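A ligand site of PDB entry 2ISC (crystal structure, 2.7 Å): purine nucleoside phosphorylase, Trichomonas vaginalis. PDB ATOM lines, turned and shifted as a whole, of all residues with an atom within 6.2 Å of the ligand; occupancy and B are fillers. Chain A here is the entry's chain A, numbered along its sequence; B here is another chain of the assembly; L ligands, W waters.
A nitrogen (N4) of the ligand lies close to the backbone NH of Gly 92 (3.3 Å). The side-chain carboxylate (OE1) of Glu 181 sits at hydrogen-bond distance from an oxygen (O2) of the ligand (2.7 Å). NE2 of His 4 of chain B is in hydrogen-bond range of O1 of the ligand, at 2.8 Å. O of Val 178 lies close to N3 of the ligand, 3.5 Å away. The side-chain carboxylate (OD2) of Asp 204 sits at hydrogen-bond distance from a nitrogen (N4) of the ligand, at 2.8 Å.
O of Cys 91 sits at hydrogen-bond distance from N of Ser 203 (3.1 Å). OE2 of Glu 179 is in hydrogen-bond range of N of Glu 181 (3.1 Å). O of Thr 90 lies within hydrogen-bond range of NH2 of Arg 87, 3.2 Å away. The backbone NH (N) of Gly 65 lies within hydrogen-bond range of the side-chain carboxylate (OE1) of Glu 181 (2.8 Å). The side-chain hydroxyl (OG) of Ser 203 lies within hydrogen-bond range of the side-chain carboxylate (OD2) of Asp 204 (2.9 Å). The backbone NH (N) of Ile 206 sits at hydrogen-bond distance from the backbone carbonyl oxygen (O) of Ala 93 (3.0 Å). The backbone NH of Val 178 sits at hydrogen-bond distance from the backbone carbonyl oxygen of Gly 92 (2.6 Å). N of Leu 158 sits at hydrogen-bond distance from OG1 of Thr 156 (3.0 Å).
Met 64 touches the ligand (CG to O2, 3.3 Å). Thr 90 touches the ligand. C of Cys 91 touches C5 of the ligand, at 3.3 Å. Thr 156 touches the ligand. CD1 of Phe 159 touches N1 of the ligand (3.4 Å). Glu 179 touches the ligand (CA to N3, 3.6 Å). SD of Met 180 touches C11 of the ligand, at 3.6 Å. OG of Ser 203 touches C5 of the ligand (3.6 Å). CG2 of Ile 206 touches N2 of the ligand, at 3.9 Å. NH2 of Arg 43 of chain B touches C8 of the ligand (3.8 Å). The nearest printed residue that does not touch the ligand is Arg 87 (4.2 Å).
Water W1 bridges N1 of the ligand (2.8 Å) and O of Phe 159 (2.8 Å).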
ATOM      1  N   GLY A  20      22.655 -31.413   4.216  1.00  0.00           N
ATOM      2  CA  GLY A  20      21.279 -31.666   3.778  1.00  0.00           C
ATOM      3  C   GLY A  20      20.914 -31.261   2.363  1.00  0.00           C
ATOM      4  O   GLY A  20      20.203 -32.003   1.659  1.00  0.00           O
ATOM      5  N   HIS A  62      22.918 -35.514   2.157  1.00  0.00           N
ATOM      6  CA  HIS A  62      22.400 -36.591   3.014  1.00  0.00           C
ATOM      7  C   HIS A  62      20.900 -36.532   3.245  1.00  0.00           C
ATOM      8  O   HIS A  62      20.379 -37.307   4.035  1.00  0.00           O
ATOM      9  CB  HIS A  62      23.153 -36.671   4.368  1.00  0.00           C
ATOM     10  CG  HIS A  62      23.049 -35.431   5.210  1.00  0.00           C
ATOM     11  ND1 HIS A  62      21.874 -34.762   5.434  1.00  0.00           N
ATOM     12  CD2 HIS A  62      23.997 -34.768   5.917  1.00  0.00           C
ATOM     13  CE1 HIS A  62      22.094 -33.724   6.232  1.00  0.00           C
ATOM     14  NE2 HIS A  62      23.374 -33.701   6.534  1.00  0.00           N
ATOM     15  N   GLY A  63      20.210 -35.634   2.556  1.00  0.00           N
ATOM     16  CA  GLY A  63      18.772 -35.417   2.762  1.00  0.00           C
ATOM     17  C   GLY A  63      18.470 -34.900   4.146  1.00  0.00           C
ATOM     18  O   GLY A  63      19.326 -34.922   5.021  1.00  0.00           O
ATOM     19  N   MET A  64      17.262 -34.420   4.373  1.00  0.00           N
ATOM     20  CA  MET A  64      16.863 -34.020   5.719  1.00  0.00           C
ATOM     21  C   MET A  64      16.323 -35.192   6.513  1.00  0.00           C
ATOM     22  O   MET A  64      15.594 -36.027   5.980  1.00  0.00           O
ATOM     23  CB  MET A  64      15.815 -32.918   5.662  1.00  0.00           C
ATOM     24  CG  MET A  64      16.174 -31.759   4.722  1.00  0.00           C
ATOM     25  SD  MET A  64      14.888 -30.516   4.716  1.00  0.00           S
ATOM     26  CE  MET A  64      13.481 -31.421   4.081  1.00  0.00           C
ATOM     27  N   GLY A  65      16.710 -35.282   7.779  1.00  0.00           N
ATOM     28  CA  GLY A  65      16.151 -36.280   8.701  1.00  0.00           C
ATOM     29  C   GLY A  65      17.009 -37.493   9.020  1.00  0.00           C
ATOM     30  O   GLY A  65      17.776 -37.988   8.187  1.00  0.00           O
ATOM     31  N   ARG A  87      29.425 -33.567   9.406  1.00  0.00           N
ATOM     32  CA  ARG A  87      28.235 -32.921   8.902  1.00  0.00           C
ATOM     33  C   ARG A  87      28.485 -31.433   8.971  1.00  0.00           C
ATOM     34  O   ARG A  87      28.807 -30.896  10.023  1.00  0.00           O
ATOM     35  CB  ARG A  87      27.006 -33.291   9.738  1.00  0.00           C
ATOM     36  CG  ARG A  87      25.770 -32.451   9.420  1.00  0.00           C
ATOM     37  CD  ARG A  87      24.485 -33.004  10.035  1.00  0.00           C
ATOM     38  NE  ARG A  87      23.563 -31.935  10.420  1.00  0.00           N
ATOM     39  CZ  ARG A  87      22.977 -31.069   9.577  1.00  0.00           C
ATOM     40  NH1 ARG A  87      23.200 -31.136   8.264  1.00  0.00           N
ATOM     41  NH2 ARG A  87      22.165 -30.142  10.058  1.00  0.00           N
ATOM     42  N   GLY A  89      26.309 -28.373   8.335  1.00  0.00           N
ATOM     43  CA  GLY A  89      24.926 -28.005   8.034  1.00  0.00           C
ATOM     44  C   GLY A  89      24.480 -26.649   8.506  1.00  0.00           C
ATOM     45  O   GLY A  89      25.279 -25.714   8.594  1.00  0.00           O
ATOM     46  N   THR A  90      23.181 -26.531   8.757  1.00  0.00           N
ATOM     47  CA  THR A  90      22.599 -25.341   9.358  1.00  0.00           C
ATOM     48  C   THR A  90      21.910 -25.815  10.617  1.00  0.00           C
ATOM     49  O   THR A  90      21.881 -27.017  10.880  1.00  0.00           O
ATOM     50  CB  THR A  90      21.588 -24.637   8.439  1.00  0.00           C
ATOM     51  OG1 THR A  90      20.592 -25.567   8.020  1.00  0.00           O
ATOM     52  CG2 THR A  90      22.284 -24.039   7.217  1.00  0.00           C
ATOM     53  N   CYS A  91      21.367 -24.886  11.390  1.00  0.00           N
ATOM     54  CA  CYS A  91      20.654 -25.256  12.603  1.00  0.00           C
ATOM     55  C   CYS A  91      19.802 -24.123  13.148  1.00  0.00           C
ATOM     56  O   CYS A  91      20.029 -22.945  12.846  1.00  0.00           O
ATOM     57  CB  CYS A  91      21.618 -25.803  13.681  1.00  0.00           C
ATOM     58  SG  CYS A  91      23.116 -24.821  13.982  1.00  0.00           S
ATOM     59  N   GLY A  92      18.783 -24.498  13.909  1.00  0.00           N
ATOM     60  CA  GLY A  92      17.895 -23.548  14.549  1.00  0.00           C
ATOM     61  C   GLY A  92      18.379 -23.344  15.957  1.00  0.00           C
ATOM     62  O   GLY A  92      18.353 -24.257  16.763  1.00  0.00           O
ATOM     63  N   ALA A  93      18.847 -22.133  16.231  1.00  0.00           N
ATOM     64  CA  ALA A  93      19.366 -21.774  17.545  1.00  0.00           C
ATOM     65  C   ALA A  93      18.323 -21.924  18.646  1.00  0.00           C
ATOM     66  O   ALA A  93      17.141 -21.626  18.449  1.00  0.00           O
ATOM     67  CB  ALA A  93      19.869 -20.353  17.506  1.00  0.00           C
ATOM     68  N   THR A 156      15.845 -33.336  15.763  1.00  0.00           N
ATOM     69  CA  THR A 156      14.378 -33.504  15.828  1.00  0.00           C
ATOM     70  C   THR A 156      13.828 -34.266  14.619  1.00  0.00           C
ATOM     71  O   THR A 156      14.361 -34.139  13.508  1.00  0.00           O
ATOM     72  CB  THR A 156      13.652 -32.153  15.980  1.00  0.00           C
ATOM     73  OG1 THR A 156      12.256 -32.383  16.144  1.00  0.00           O
ATOM     74  CG2 THR A 156      13.860 -31.279  14.778  1.00  0.00           C
ATOM     75  N   LEU A 158      10.592 -33.823  14.053  1.00  0.00           N
ATOM     76  CA  LEU A 158       9.497 -32.912  13.757  1.00  0.00           C
ATOM     77  C   LEU A 158       9.942 -31.450  13.655  1.00  0.00           C
ATOM     78  O   LEU A 158       9.966 -30.733  14.660  1.00  0.00           O
ATOM     79  CB  LEU A 158       8.428 -33.049  14.824  1.00  0.00           C
ATOM     80  CG  LEU A 158       7.215 -33.937  14.512  1.00  0.00           C
ATOM     81  CD1 LEU A 158       7.283 -34.651  13.137  1.00  0.00           C
ATOM     82  CD2 LEU A 158       7.008 -34.897  15.679  1.00  0.00           C
ATOM     83  N   PHE A 159      10.285 -31.035  12.436  1.00  0.00           N
ATOM     84  CA  PHE A 159      10.656 -29.666  12.142  1.00  0.00           C
ATOM     85  C   PHE A 159       9.554 -28.728  12.627  1.00  0.00           C
ATOM     86  O   PHE A 159       9.825 -27.778  13.341  1.00  0.00           O
ATOM     87  CB  PHE A 159      10.902 -29.492  10.644  1.00  0.00           C
ATOM     88  CG  PHE A 159      11.262 -28.088  10.250  1.00  0.00           C
ATOM     89  CD1 PHE A 159      12.576 -27.643  10.336  1.00  0.00           C
ATOM     90  CD2 PHE A 159      10.284 -27.203   9.798  1.00  0.00           C
ATOM     91  CE1 PHE A 159      12.918 -26.342   9.967  1.00  0.00           C
ATOM     92  CE2 PHE A 159      10.623 -25.894   9.441  1.00  0.00           C
ATOM     93  CZ  PHE A 159      11.936 -25.463   9.528  1.00  0.00           C
ATOM     94  N   VAL A 178      19.139 -26.720  17.119  1.00  0.00           N
ATOM     95  CA  VAL A 178      18.354 -27.829  16.590  1.00  0.00           C
ATOM     96  C   VAL A 178      18.730 -28.121  15.151  1.00  0.00           C
ATOM     97  O   VAL A 178      18.716 -27.228  14.314  1.00  0.00           O
ATOM     98  CB  VAL A 178      16.826 -27.541  16.621  1.00  0.00           C
ATOM     99  CG1 VAL A 178      16.044 -28.776  16.228  1.00  0.00           C
ATOM    100  CG2 VAL A 178      16.394 -27.116  17.985  1.00  0.00           C
ATOM    101  N   GLU A 179      19.063 -29.358  14.857  1.00  0.00           N
ATOM    102  CA  GLU A 179      19.029 -29.817  13.476  1.00  0.00           C
ATOM    103  C   GLU A 179      18.198 -31.103  13.402  1.00  0.00           C
ATOM    104  O   GLU A 179      17.305 -31.305  14.232  1.00  0.00           O
ATOM    105  CB  GLU A 179      20.429 -29.981  12.875  1.00  0.00           C
ATOM    106  CG  GLU A 179      21.448 -30.571  13.802  1.00  0.00           C
ATOM    107  CD  GLU A 179      21.305 -32.055  13.981  1.00  0.00           C
ATOM    108  OE1 GLU A 179      20.470 -32.487  14.823  1.00  0.00           O
ATOM    109  OE2 GLU A 179      22.037 -32.793  13.289  1.00  0.00           O
ATOM    110  N   MET A 180      18.481 -31.973  12.437  1.00  0.00           N
ATOM    111  CA  MET A 180      17.621 -33.110  12.239  1.00  0.00           C
ATOM    112  C   MET A 180      18.363 -34.371  11.883  1.00  0.00           C
ATOM    113  O   MET A 180      17.782 -35.264  11.287  1.00  0.00           O
ATOM    114  CB  MET A 180      16.574 -32.813  11.159  1.00  0.00           C
ATOM    115  CG  MET A 180      15.548 -31.759  11.545  1.00  0.00           C
ATOM    116  SD  MET A 180      14.329 -31.423  10.258  1.00  0.00           S
ATOM    117  CE  MET A 180      13.402 -32.955  10.328  1.00  0.00           C
ATOM    118  N   GLU A 181      19.643 -34.450  12.251  1.00  0.00           N
ATOM    119  CA  GLU A 181      20.521 -35.466  11.673  1.00  0.00           C
ATOM    120  C   GLU A 181      21.605 -36.049  12.568  1.00  0.00           C
ATOM    121  O   GLU A 181      21.950 -37.219  12.425  1.00  0.00           O
ATOM    122  CB  GLU A 181      21.191 -34.920  10.410  1.00  0.00           C
ATOM    123  CG  GLU A 181      20.271 -34.761   9.205  1.00  0.00           C
ATOM    124  CD  GLU A 181      19.570 -33.419   9.147  1.00  0.00           C
ATOM    125  OE1 GLU A 181      18.575 -33.328   8.409  1.00  0.00           O
ATOM    126  OE2 GLU A 181      20.007 -32.462   9.811  1.00  0.00           O
ATOM    127  N   SER A 203      20.919 -20.453  11.171  1.00  0.00           N
ATOM    128  CA  SER A 203      20.127 -19.852  10.108  1.00  0.00           C
ATOM    129  C   SER A 203      18.861 -19.157  10.601  1.00  0.00           C
ATOM    130  O   SER A 203      18.339 -18.276   9.933  1.00  0.00           O
ATOM    131  CB  SER A 203      19.765 -20.893   9.034  1.00  0.00           C
ATOM    132  OG  SER A 203      19.061 -22.001   9.579  1.00  0.00           O
ATOM    133  N   ASP A 204      18.378 -19.553  11.769  1.00  0.00           N
ATOM    134  CA  ASP A 204      17.131 -19.046  12.332  1.00  0.00           C
ATOM    135  C   ASP A 204      17.100 -19.357  13.816  1.00  0.00           C
ATOM    136  O   ASP A 204      17.750 -20.298  14.266  1.00  0.00           O
ATOM    137  CB  ASP A 204      15.927 -19.699  11.639  1.00  0.00           C
ATOM    138  CG  ASP A 204      15.900 -21.212  11.808  1.00  0.00           C
ATOM    139  OD1 ASP A 204      15.138 -21.712  12.656  1.00  0.00           O
ATOM    140  OD2 ASP A 204      16.625 -21.909  11.084  1.00  0.00           O
ATOM    141  N   ILE A 206      14.744 -20.442  17.112  1.00  0.00           N
ATOM    142  CA  ILE A 206      13.425 -20.991  17.456  1.00  0.00           C
ATOM    143  C   ILE A 206      12.807 -20.307  18.690  1.00  0.00           C
ATOM    144  O   ILE A 206      11.710 -20.679  19.126  1.00  0.00           O
ATOM    145  CB  ILE A 206      13.376 -22.574  17.526  1.00  0.00           C
ATOM    146  CG1 ILE A 206      13.318 -23.113  18.963  1.00  0.00           C
ATOM    147  CG2 ILE A 206      14.470 -23.214  16.645  1.00  0.00           C
ATOM    148  CD1 ILE A 206      14.637 -23.153  19.715  1.00  0.00           C
ATOM    149  N   PRO B   3      10.809 -22.187   4.076  1.00  0.00           N
ATOM    150  CA  PRO B   3      12.243 -22.499   4.011  1.00  0.00           C
ATOM    151  C   PRO B   3      12.601 -23.623   3.036  1.00  0.00           C
ATOM    152  O   PRO B   3      13.786 -23.808   2.732  1.00  0.00           O
ATOM    153  CB  PRO B   3      12.559 -22.914   5.447  1.00  0.00           C
ATOM    154  CG  PRO B   3      11.504 -22.265   6.280  1.00  0.00           C
ATOM    155  CD  PRO B   3      10.276 -22.380   5.441  1.00  0.00           C
ATOM    156  N   HIS B   4      11.610 -24.354   2.527  1.00  0.00           N
ATOM    157  CA  HIS B   4      11.874 -25.534   1.683  1.00  0.00           C
ATOM    158  C   HIS B   4      11.217 -25.462   0.307  1.00  0.00           C
ATOM    159  O   HIS B   4      11.160 -26.461  -0.404  1.00  0.00           O
ATOM    160  CB  HIS B   4      11.383 -26.794   2.376  1.00  0.00           C
ATOM    161  CG  HIS B   4      11.872 -26.939   3.779  1.00  0.00           C
ATOM    162  ND1 HIS B   4      11.162 -26.466   4.864  1.00  0.00           N
ATOM    163  CD2 HIS B   4      13.015 -27.490   4.273  1.00  0.00           C
ATOM    164  CE1 HIS B   4      11.836 -26.736   5.969  1.00  0.00           C
ATOM    165  NE2 HIS B   4      12.956 -27.346   5.635  1.00  0.00           N
ATOM    166  N   ARG B  43      16.742 -27.008  -2.590  1.00  0.00           N
ATOM    167  CA  ARG B  43      17.364 -28.306  -2.281  1.00  0.00           C
ATOM    168  C   ARG B  43      17.151 -29.365  -3.373  1.00  0.00           C
ATOM    169  O   ARG B  43      17.156 -30.567  -3.083  1.00  0.00           O
ATOM    170  CB  ARG B  43      16.904 -28.846  -0.932  1.00  0.00           C
ATOM    171  CG  ARG B  43      17.370 -28.019   0.226  1.00  0.00           C
ATOM    172  CD  ARG B  43      16.504 -28.223   1.431  1.00  0.00           C
ATOM    173  NE  ARG B  43      16.948 -27.378   2.525  1.00  0.00           N
ATOM    174  CZ  ARG B  43      17.904 -27.719   3.398  1.00  0.00           C
ATOM    175  NH1 ARG B  43      18.496 -28.916   3.313  1.00  0.00           N
ATOM    176  NH2 ARG B  43      18.242 -26.877   4.359  1.00  0.00           N
ATOM    177  N   ILE B  71       7.853 -32.559   6.696  1.00  0.00           N
ATOM    178  CA  ILE B  71       8.099 -31.160   6.320  1.00  0.00           C
ATOM    179  C   ILE B  71       7.262 -30.789   5.090  1.00  0.00           C
ATOM    180  O   ILE B  71       6.487 -29.826   5.126  1.00  0.00           O
ATOM    181  CB  ILE B  71       9.616 -30.903   6.061  1.00  0.00           C
ATOM    182  CG1 ILE B  71      10.374 -30.709   7.378  1.00  0.00           C
ATOM    183  CG2 ILE B  71       9.861 -29.699   5.147  1.00  0.00           C
ATOM    184  CD1 ILE B  71      11.855 -30.924   7.228  1.00  0.00           C
HETATM  185  N1  LIG L   1      14.409 -26.911  13.093  1.00  0.00           N
HETATM  186  C1  LIG L   1      15.082 -28.187  12.765  1.00  0.00           C
HETATM  187  C2  LIG L   1      16.739 -26.843  11.542  1.00  0.00           C
HETATM  188  C3  LIG L   1      16.116 -25.657  11.850  1.00  0.00           C
HETATM  189  C4  LIG L   1      14.881 -25.708  12.676  1.00  0.00           C
HETATM  190  C5  LIG L   1      17.873 -25.179  10.628  1.00  0.00           C
HETATM  191  N2  LIG L   1      14.286 -24.645  12.974  1.00  0.00           N
HETATM  192  N3  LIG L   1      16.298 -28.063  11.952  1.00  0.00           N
HETATM  193  C6  LIG L   1      17.845 -26.567  10.759  1.00  0.00           C
HETATM  194  N4  LIG L   1      16.821 -24.650  11.289  1.00  0.00           N
HETATM  195  C7  LIG L   1      18.880 -27.541  10.228  1.00  0.00           C
HETATM  196  N5  LIG L   1      18.580 -28.311   9.028  1.00  0.00           N
HETATM  197  C8  LIG L   1      17.697 -27.618   8.063  1.00  0.00           C
HETATM  198  C9  LIG L   1      16.766 -28.691   7.505  1.00  0.00           C
HETATM  199  C10 LIG L   1      15.295 -28.283   7.589  1.00  0.00           C
HETATM  200  O1  LIG L   1      15.080 -26.875   7.407  1.00  0.00           O
HETATM  201  C11 LIG L   1      17.039 -29.959   8.306  1.00  0.00           C
HETATM  202  O2  LIG L   1      17.764 -30.908   7.525  1.00  0.00           O
HETATM  203  C12 LIG L   1      17.945 -29.566   9.457  1.00  0.00           C
HETATM  204  O   HOH W   1      12.263 -27.596  14.744  1.00  0.00           O
HETATM  205  O   HOH W   2      15.952 -24.504   6.894  1.00  0.00           O
